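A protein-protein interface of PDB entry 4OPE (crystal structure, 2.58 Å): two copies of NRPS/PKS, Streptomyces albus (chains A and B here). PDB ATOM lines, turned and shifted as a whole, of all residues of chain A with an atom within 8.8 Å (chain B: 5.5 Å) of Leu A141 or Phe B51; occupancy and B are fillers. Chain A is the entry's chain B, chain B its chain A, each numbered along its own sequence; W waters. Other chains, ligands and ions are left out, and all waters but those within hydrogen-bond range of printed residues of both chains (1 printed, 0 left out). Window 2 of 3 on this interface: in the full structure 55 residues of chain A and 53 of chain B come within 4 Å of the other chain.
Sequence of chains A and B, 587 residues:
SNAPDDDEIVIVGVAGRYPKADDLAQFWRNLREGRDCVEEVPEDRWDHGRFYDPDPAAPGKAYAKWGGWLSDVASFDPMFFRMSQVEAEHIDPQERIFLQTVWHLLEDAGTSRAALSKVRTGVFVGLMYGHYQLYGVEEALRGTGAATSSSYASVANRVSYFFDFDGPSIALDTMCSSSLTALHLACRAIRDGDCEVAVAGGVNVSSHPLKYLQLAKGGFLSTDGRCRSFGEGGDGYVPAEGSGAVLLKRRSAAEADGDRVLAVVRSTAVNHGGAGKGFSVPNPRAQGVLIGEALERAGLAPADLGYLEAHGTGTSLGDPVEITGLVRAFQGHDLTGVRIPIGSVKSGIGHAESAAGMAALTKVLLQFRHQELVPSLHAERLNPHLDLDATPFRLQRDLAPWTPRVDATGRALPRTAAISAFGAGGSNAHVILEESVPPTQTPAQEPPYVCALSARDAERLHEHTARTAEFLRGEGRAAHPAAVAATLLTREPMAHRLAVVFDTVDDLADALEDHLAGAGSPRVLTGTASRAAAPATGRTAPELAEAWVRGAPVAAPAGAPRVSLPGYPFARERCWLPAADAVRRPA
The backbone carbonyl oxygen (O) of Phe B51 lies within hydrogen-bond range of the backbone NH (N) of Ala B62 (2.9 Å).
ND1 of His B208 lies within hydrogen-bond range of N of Leu B210, 3.0 Å away.
Ala A140 touches Leu B213 (O to CD1, 3.1 Å).
CD1 of Phe B51 touches O of Leu A141 (3.6 Å).
CA of Leu A141 touches CD1 of Leu B213 (3.9 Å).
O of Gly B60 touches CA of Gly A143, 3.5 Å away.
Leu B210 touches Ala A147 (CD2 to CB, 3.7 Å).
Of chain B, only Phe B51 and Leu B213 come within 4 Å of Leu A141.
No residue of chain A comes within 4 Å of Gly B49.
Ala B62 touches none of the printed residues of chain A.
Of the printed residues of chain B, Ala A140 touches Leu B213 (3.1 Å).
Of the printed residues of chain A, Leu B210 touches Ala A147 (3.7 Å).
Of the printed residues of chain B, Ala A147 touches Leu B210 (3.7 Å).
Of the printed residues of chain A, Gly B60 touches Gly A143.
The nearest residue of chain B that does not touch Leu A141 is His B208 (4.05 Å).
Of the 12 printed residues of chain A, 4 touch a printed residue of chain B.
Printed residues of chain A that touch a printed residue of chain B: Ala A140, Leu A141, Gly A143 and Ala A147.
Hydrophobic or aromatic side chains of chain A within 4 Å of the printed part of chain B: Leu A141 and Ala A147.
Hydrophobic or aromatic side chains of chain B that line the printed part of chain A: Phe B51, Leu B210 and Leu B213.
Among the printed residues, 5 pairs touch across the chains.
Among the printed residues, no Asp or Glu carboxylate lies within 4 Å of a Lys or Arg side-chain nitrogen of the other chain.
No position is printed for both chains.
Of the 5 pairs that touch across the chains among the printed residues, none has its exchanged pair printed and touching as well.
Water W1 lies within hydrogen-bond range of the backbone carbonyl oxygen (O) of Leu A141 (2.7 Å), the backbone carbonyl oxygen (O) of Gly B60 (2.8 Å) and the side-chain amino group (NZ) of Lys B61 (3.0 Å).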
ATOM      1  N   GLY A 136     -21.410   6.768 -28.140  1.00  0.00           N
ATOM      2  CA  GLY A 136     -19.944   6.833 -28.001  1.00  0.00           C
ATOM      3  C   GLY A 136     -19.444   6.196 -26.727  1.00  0.00           C
ATOM      4  O   GLY A 136     -18.292   6.319 -26.351  1.00  0.00           O
ATOM      5  N   VAL A 137     -20.331   5.502 -26.057  1.00  0.00           N
ATOM      6  CA  VAL A 137     -20.014   4.917 -24.779  1.00  0.00           C
ATOM      7  C   VAL A 137     -19.039   3.767 -24.992  1.00  0.00           C
ATOM      8  O   VAL A 137     -18.024   3.674 -24.298  1.00  0.00           O
ATOM      9  CB  VAL A 137     -21.316   4.450 -24.091  1.00  0.00           C
ATOM     10  CG1 VAL A 137     -21.021   3.600 -22.870  1.00  0.00           C
ATOM     11  CG2 VAL A 137     -22.184   5.666 -23.749  1.00  0.00           C
ATOM     12  N   GLU A 138     -19.334   2.918 -25.969  1.00  0.00           N
ATOM     13  CA  GLU A 138     -18.441   1.830 -26.308  1.00  0.00           C
ATOM     14  C   GLU A 138     -17.049   2.353 -26.677  1.00  0.00           C
ATOM     15  O   GLU A 138     -16.063   1.827 -26.221  1.00  0.00           O
ATOM     16  CB  GLU A 138     -19.026   0.973 -27.426  1.00  0.00           C
ATOM     17  CG  GLU A 138     -18.442  -0.439 -27.486  1.00  0.00           C
ATOM     18  CD  GLU A 138     -18.605  -1.140 -28.860  1.00  0.00           C
ATOM     19  OE1 GLU A 138     -17.614  -1.758 -29.351  1.00  0.00           O
ATOM     20  OE2 GLU A 138     -19.716  -1.084 -29.451  1.00  0.00           O
ATOM     21  N   GLU A 139     -16.968   3.422 -27.443  1.00  0.00           N
ATOM     22  CA  GLU A 139     -15.668   3.951 -27.867  1.00  0.00           C
ATOM     23  C   GLU A 139     -14.898   4.525 -26.697  1.00  0.00           C
ATOM     24  O   GLU A 139     -13.713   4.246 -26.510  1.00  0.00           O
ATOM     25  CB  GLU A 139     -15.828   5.039 -28.941  1.00  0.00           C
ATOM     26  CG  GLU A 139     -16.223   4.533 -30.327  1.00  0.00           C
ATOM     27  CD  GLU A 139     -17.715   4.220 -30.469  1.00  0.00           C
ATOM     28  OE1 GLU A 139     -18.482   4.515 -29.507  1.00  0.00           O
ATOM     29  OE2 GLU A 139     -18.132   3.664 -31.538  1.00  0.00           O
ATOM     30  N   ALA A 140     -15.571   5.330 -25.901  1.00  0.00           N
ATOM     31  CA  ALA A 140     -14.908   5.993 -24.781  1.00  0.00           C
ATOM     32  C   ALA A 140     -14.369   5.001 -23.749  1.00  0.00           C
ATOM     33  O   ALA A 140     -13.297   5.216 -23.192  1.00  0.00           O
ATOM     34  CB  ALA A 140     -15.844   6.995 -24.121  1.00  0.00           C
ATOM     35  N   LEU A 141     -15.121   3.936 -23.493  1.00  0.00           N
ATOM     36  CA  LEU A 141     -14.658   2.838 -22.639  1.00  0.00           C
ATOM     37  C   LEU A 141     -13.451   2.096 -23.243  1.00  0.00           C
ATOM     38  O   LEU A 141     -12.593   1.572 -22.522  1.00  0.00           O
ATOM     39  CB  LEU A 141     -15.782   1.810 -22.420  1.00  0.00           C
ATOM     40  CG  LEU A 141     -16.990   2.176 -21.567  1.00  0.00           C
ATOM     41  CD1 LEU A 141     -17.876   0.960 -21.329  1.00  0.00           C
ATOM     42  CD2 LEU A 141     -16.554   2.761 -20.244  1.00  0.00           C
ATOM     43  N   ARG A 142     -13.413   2.010 -24.567  1.00  0.00           N
ATOM     44  CA  ARG A 142     -12.338   1.300 -25.211  1.00  0.00           C
ATOM     45  C   ARG A 142     -11.118   2.196 -25.273  1.00  0.00           C
ATOM     46  O   ARG A 142     -10.011   1.708 -25.435  1.00  0.00           O
ATOM     47  CB  ARG A 142     -12.741   0.807 -26.596  1.00  0.00           C
ATOM     48  CG  ARG A 142     -13.763  -0.338 -26.587  1.00  0.00           C
ATOM     49  CD  ARG A 142     -14.197  -0.715 -28.008  1.00  0.00           C
ATOM     50  NE  ARG A 142     -13.031  -0.951 -28.881  1.00  0.00           N
ATOM     51  CZ  ARG A 142     -12.566  -0.127 -29.836  1.00  0.00           C
ATOM     52  NH1 ARG A 142     -13.171   1.036 -30.123  1.00  0.00           N
ATOM     53  NH2 ARG A 142     -11.482  -0.477 -30.538  1.00  0.00           N
ATOM     54  N   GLY A 143     -11.316   3.497 -25.124  1.00  0.00           N
ATOM     55  CA  GLY A 143     -10.207   4.414 -25.098  1.00  0.00           C
ATOM     56  C   GLY A 143     -10.005   5.117 -26.415  1.00  0.00           C
ATOM     57  O   GLY A 143      -9.096   5.916 -26.537  1.00  0.00           O
ATOM     58  N   THR A 144     -10.850   4.859 -27.404  1.00  0.00           N
ATOM     59  CA  THR A 144     -10.620   5.433 -28.736  1.00  0.00           C
ATOM     60  C   THR A 144     -11.423   6.687 -29.003  1.00  0.00           C
ATOM     61  O   THR A 144     -11.289   7.284 -30.062  1.00  0.00           O
ATOM     62  CB  THR A 144     -10.896   4.412 -29.860  1.00  0.00           C
ATOM     63  OG1 THR A 144     -12.255   3.990 -29.813  1.00  0.00           O
ATOM     64  CG2 THR A 144      -9.976   3.205 -29.705  1.00  0.00           C
ATOM     65  N   GLY A 145     -12.272   7.071 -28.057  1.00  0.00           N
ATOM     66  CA  GLY A 145     -13.111   8.262 -28.202  1.00  0.00           C
ATOM     67  C   GLY A 145     -13.228   8.944 -26.859  1.00  0.00           C
ATOM     68  O   GLY A 145     -12.727   8.449 -25.835  1.00  0.00           O
ATOM     69  N   ALA A 146     -13.882  10.094 -26.880  1.00  0.00           N
ATOM     70  CA  ALA A 146     -14.222  10.822 -25.686  1.00  0.00           C
ATOM     71  C   ALA A 146     -15.710  10.700 -25.475  1.00  0.00           C
ATOM     72  O   ALA A 146     -16.466  10.573 -26.436  1.00  0.00           O
ATOM     73  CB  ALA A 146     -13.850  12.270 -25.858  1.00  0.00           C
ATOM     74  N   ALA A 147     -16.136  10.780 -24.216  1.00  0.00           N
ATOM     75  CA  ALA A 147     -17.550  10.647 -23.872  1.00  0.00           C
ATOM     76  C   ALA A 147     -18.337  11.857 -24.285  1.00  0.00           C
ATOM     77  O   ALA A 147     -17.812  12.964 -24.270  1.00  0.00           O
ATOM     78  CB  ALA A 147     -17.709  10.445 -22.381  1.00  0.00           C
ATOM     79  N   TRP B  46     -16.745  -2.642 -11.152  1.00  0.00           N
ATOM     80  CA  TRP B  46     -16.187  -2.819 -12.480  1.00  0.00           C
ATOM     81  C   TRP B  46     -14.703  -3.079 -12.341  1.00  0.00           C
ATOM     82  O   TRP B  46     -14.119  -2.857 -11.267  1.00  0.00           O
ATOM     83  CB  TRP B  46     -16.467  -1.625 -13.413  1.00  0.00           C
ATOM     84  CG  TRP B  46     -15.799  -0.342 -13.031  1.00  0.00           C
ATOM     85  CD1 TRP B  46     -14.497  -0.014 -13.214  1.00  0.00           C
ATOM     86  CD2 TRP B  46     -16.416   0.800 -12.436  1.00  0.00           C
ATOM     87  NE1 TRP B  46     -14.250   1.253 -12.743  1.00  0.00           N
ATOM     88  CE2 TRP B  46     -15.413   1.784 -12.276  1.00  0.00           C
ATOM     89  CE3 TRP B  46     -17.717   1.091 -12.022  1.00  0.00           C
ATOM     90  CZ2 TRP B  46     -15.666   3.031 -11.715  1.00  0.00           C
ATOM     91  CZ3 TRP B  46     -17.970   2.339 -11.493  1.00  0.00           C
ATOM     92  CH2 TRP B  46     -16.949   3.282 -11.325  1.00  0.00           C
ATOM     93  N   ASP B  47     -14.132  -3.592 -13.429  1.00  0.00           N
ATOM     94  CA  ASP B  47     -12.738  -3.938 -13.517  1.00  0.00           C
ATOM     95  C   ASP B  47     -12.063  -2.658 -13.939  1.00  0.00           C
ATOM     96  O   ASP B  47     -12.143  -2.240 -15.097  1.00  0.00           O
ATOM     97  CB  ASP B  47     -12.552  -5.054 -14.557  1.00  0.00           C
ATOM     98  CG  ASP B  47     -11.073  -5.413 -14.826  1.00  0.00           C
ATOM     99  OD1 ASP B  47     -10.171  -5.009 -14.051  1.00  0.00           O
ATOM    100  OD2 ASP B  47     -10.830  -6.119 -15.843  1.00  0.00           O
ATOM    101  N   HIS B  48     -11.423  -2.008 -12.985  1.00  0.00           N
ATOM    102  CA  HIS B  48     -10.781  -0.753 -13.270  1.00  0.00           C
ATOM    103  C   HIS B  48      -9.478  -0.936 -14.064  1.00  0.00           C
ATOM    104  O   HIS B  48      -9.002   0.017 -14.683  1.00  0.00           O
ATOM    105  CB  HIS B  48     -10.533   0.035 -11.993  1.00  0.00           C
ATOM    106  CG  HIS B  48     -10.414   1.502 -12.231  1.00  0.00           C
ATOM    107  ND1 HIS B  48     -11.442   2.246 -12.754  1.00  0.00           N
ATOM    108  CD2 HIS B  48      -9.390   2.364 -12.044  1.00  0.00           C
ATOM    109  CE1 HIS B  48     -11.063   3.506 -12.873  1.00  0.00           C
ATOM    110  NE2 HIS B  48      -9.819   3.607 -12.448  1.00  0.00           N
ATOM    111  N   GLY B  49      -8.910  -2.143 -14.050  1.00  0.00           N
ATOM    112  CA  GLY B  49      -7.791  -2.485 -14.945  1.00  0.00           C
ATOM    113  C   GLY B  49      -8.039  -2.080 -16.395  1.00  0.00           C
ATOM    114  O   GLY B  49      -7.197  -1.449 -17.004  1.00  0.00           O
ATOM    115  N   ARG B  50      -9.223  -2.382 -16.931  1.00  0.00           N
ATOM    116  CA  ARG B  50      -9.562  -2.029 -18.334  1.00  0.00           C
ATOM    117  C   ARG B  50      -9.442  -0.557 -18.686  1.00  0.00           C
ATOM    118  O   ARG B  50      -9.453  -0.223 -19.865  1.00  0.00           O
ATOM    119  CB  ARG B  50     -10.996  -2.423 -18.704  1.00  0.00           C
ATOM    120  CG  ARG B  50     -11.468  -3.722 -18.099  1.00  0.00           C
ATOM    121  CD  ARG B  50     -12.099  -4.622 -19.140  1.00  0.00           C
ATOM    122  NE  ARG B  50     -13.290  -4.054 -19.792  1.00  0.00           N
ATOM    123  CZ  ARG B  50     -14.522  -4.560 -19.687  1.00  0.00           C
ATOM    124  NH1 ARG B  50     -15.536  -3.990 -20.344  1.00  0.00           N
ATOM    125  NH2 ARG B  50     -14.756  -5.638 -18.924  1.00  0.00           N
ATOM    126  N   PHE B  51      -9.411   0.315 -17.677  1.00  0.00           N
ATOM    127  CA  PHE B  51      -9.555   1.759 -17.863  1.00  0.00           C
ATOM    128  C   PHE B  51      -8.471   2.585 -17.189  1.00  0.00           C
ATOM    129  O   PHE B  51      -8.444   3.808 -17.366  1.00  0.00           O
ATOM    130  CB  PHE B  51     -10.883   2.231 -17.281  1.00  0.00           C
ATOM    131  CG  PHE B  51     -12.050   1.352 -17.609  1.00  0.00           C
ATOM    132  CD1 PHE B  51     -12.534   1.263 -18.912  1.00  0.00           C
ATOM    133  CD2 PHE B  51     -12.687   0.643 -16.615  1.00  0.00           C
ATOM    134  CE1 PHE B  51     -13.619   0.456 -19.218  1.00  0.00           C
ATOM    135  CE2 PHE B  51     -13.773  -0.154 -16.918  1.00  0.00           C
ATOM    136  CZ  PHE B  51     -14.233  -0.256 -18.221  1.00  0.00           C
ATOM    137  N   TYR B  52      -7.602   1.939 -16.413  1.00  0.00           N
ATOM    138  CA  TYR B  52      -6.613   2.650 -15.624  1.00  0.00           C
ATOM    139  C   TYR B  52      -5.269   2.766 -16.340  1.00  0.00           C
ATOM    140  O   TYR B  52      -4.806   1.815 -16.974  1.00  0.00           O
ATOM    141  CB  TYR B  52      -6.396   1.907 -14.317  1.00  0.00           C
ATOM    142  CG  TYR B  52      -5.406   2.536 -13.352  1.00  0.00           C
ATOM    143  CD1 TYR B  52      -5.633   3.798 -12.813  1.00  0.00           C
ATOM    144  CD2 TYR B  52      -4.279   1.838 -12.933  1.00  0.00           C
ATOM    145  CE1 TYR B  52      -4.741   4.362 -11.918  1.00  0.00           C
ATOM    146  CE2 TYR B  52      -3.387   2.386 -12.023  1.00  0.00           C
ATOM    147  CZ  TYR B  52      -3.627   3.645 -11.526  1.00  0.00           C
ATOM    148  OH  TYR B  52      -2.762   4.174 -10.617  1.00  0.00           O
ATOM    149  N   ASP B  53      -4.651   3.938 -16.237  1.00  0.00           N
ATOM    150  CA  ASP B  53      -3.255   4.125 -16.627  1.00  0.00           C
ATOM    151  C   ASP B  53      -2.759   5.241 -15.723  1.00  0.00           C
ATOM    152  O   ASP B  53      -3.320   6.348 -15.741  1.00  0.00           O
ATOM    153  CB  ASP B  53      -3.103   4.478 -18.125  1.00  0.00           C
ATOM    154  CG  ASP B  53      -1.620   4.621 -18.576  1.00  0.00           C
ATOM    155  OD1 ASP B  53      -0.775   5.135 -17.822  1.00  0.00           O
ATOM    156  OD2 ASP B  53      -1.302   4.229 -19.723  1.00  0.00           O
ATOM    157  N   GLY B  60      -7.736   8.457 -23.271  1.00  0.00           N
ATOM    158  CA  GLY B  60      -8.827   7.486 -23.158  1.00  0.00           C
ATOM    159  C   GLY B  60      -8.718   6.610 -21.925  1.00  0.00           C
ATOM    160  O   GLY B  60      -9.201   5.452 -21.894  1.00  0.00           O
ATOM    161  N   LYS B  61      -8.104   7.200 -20.897  1.00  0.00           N
ATOM    162  CA  LYS B  61      -7.739   6.504 -19.674  1.00  0.00           C
ATOM    163  C   LYS B  61      -7.992   7.342 -18.402  1.00  0.00           C
ATOM    164  O   LYS B  61      -8.011   8.579 -18.424  1.00  0.00           O
ATOM    165  CB  LYS B  61      -6.259   6.111 -19.749  1.00  0.00           C
ATOM    166  CG  LYS B  61      -5.964   5.013 -20.735  1.00  0.00           C
ATOM    167  CD  LYS B  61      -6.894   3.855 -20.457  1.00  0.00           C
ATOM    168  CE  LYS B  61      -6.360   2.555 -21.005  1.00  0.00           C
ATOM    169  NZ  LYS B  61      -7.520   1.782 -21.493  1.00  0.00           N
ATOM    170  N   ALA B  62      -8.164   6.644 -17.289  1.00  0.00           N
ATOM    171  CA  ALA B  62      -8.263   7.301 -16.015  1.00  0.00           C
ATOM    172  C   ALA B  62      -6.967   7.136 -15.257  1.00  0.00           C
ATOM    173  O   ALA B  62      -6.442   6.060 -15.181  1.00  0.00           O
ATOM    174  CB  ALA B  62      -9.439   6.742 -15.224  1.00  0.00           C
ATOM    175  N   HIS B 208     -21.195   3.556 -13.052  1.00  0.00           N
ATOM    176  CA  HIS B 208     -20.588   3.240 -14.316  1.00  0.00           C
ATOM    177  C   HIS B 208     -19.202   3.862 -14.439  1.00  0.00           C
ATOM    178  O   HIS B 208     -18.997   4.993 -14.028  1.00  0.00           O
ATOM    179  CB  HIS B 208     -21.498   3.779 -15.394  1.00  0.00           C
ATOM    180  CG  HIS B 208     -21.285   3.181 -16.746  1.00  0.00           C
ATOM    181  ND1 HIS B 208     -20.205   3.498 -17.527  1.00  0.00           N
ATOM    182  CD2 HIS B 208     -22.044   2.345 -17.484  1.00  0.00           C
ATOM    183  CE1 HIS B 208     -20.288   2.869 -18.682  1.00  0.00           C
ATOM    184  NE2 HIS B 208     -21.403   2.167 -18.685  1.00  0.00           N
ATOM    185  N   PRO B 209     -18.245   3.117 -14.995  1.00  0.00           N
ATOM    186  CA  PRO B 209     -16.870   3.582 -15.192  1.00  0.00           C
ATOM    187  C   PRO B 209     -16.681   4.778 -16.136  1.00  0.00           C
ATOM    188  O   PRO B 209     -15.668   5.441 -16.077  1.00  0.00           O
ATOM    189  CB  PRO B 209     -16.169   2.343 -15.778  1.00  0.00           C
ATOM    190  CG  PRO B 209     -17.255   1.483 -16.343  1.00  0.00           C
ATOM    191  CD  PRO B 209     -18.402   1.703 -15.405  1.00  0.00           C
ATOM    192  N   LEU B 210     -17.626   5.030 -17.024  1.00  0.00           N
ATOM    193  CA  LEU B 210     -17.615   6.209 -17.914  1.00  0.00           C
ATOM    194  C   LEU B 210     -17.317   7.485 -17.167  1.00  0.00           C
ATOM    195  O   LEU B 210     -16.517   8.285 -17.631  1.00  0.00           O
ATOM    196  CB  LEU B 210     -18.958   6.309 -18.616  1.00  0.00           C
ATOM    197  CG  LEU B 210     -19.300   7.191 -19.839  1.00  0.00           C
ATOM    198  CD1 LEU B 210     -19.473   8.648 -19.472  1.00  0.00           C
ATOM    199  CD2 LEU B 210     -18.265   7.041 -20.918  1.00  0.00           C
ATOM    200  N   LEU B 213     -13.704   8.121 -16.735  1.00  0.00           N
ATOM    201  CA  LEU B 213     -13.040   8.603 -17.960  1.00  0.00           C
ATOM    202  C   LEU B 213     -13.329  10.058 -18.285  1.00  0.00           C
ATOM    203  O   LEU B 213     -12.429  10.833 -18.555  1.00  0.00           O
ATOM    204  CB  LEU B 213     -13.361   7.729 -19.170  1.00  0.00           C
ATOM    205  CG  LEU B 213     -12.772   6.333 -19.003  1.00  0.00           C
ATOM    206  CD1 LEU B 213     -13.265   5.501 -20.137  1.00  0.00           C
ATOM    207  CD2 LEU B 213     -11.257   6.310 -18.993  1.00  0.00           C
ATOM    208  N   VAL B 583     -18.735  -4.995 -17.608  1.00  0.00           N
ATOM    209  CA  VAL B 583     -17.623  -4.110 -17.211  1.00  0.00           C
ATOM    210  C   VAL B 583     -16.749  -4.705 -16.104  1.00  0.00           C
ATOM    211  O   VAL B 583     -15.748  -4.125 -15.711  1.00  0.00           O
ATOM    212  CB  VAL B 583     -18.090  -2.646 -16.858  1.00  0.00           C
ATOM    213  CG1 VAL B 583     -18.768  -1.990 -18.061  1.00  0.00           C
ATOM    214  CG2 VAL B 583     -19.013  -2.578 -15.623  1.00  0.00           C
HETATM  215  O   HOH W   1     -10.307   2.845 -21.739  1.00  0.00           O
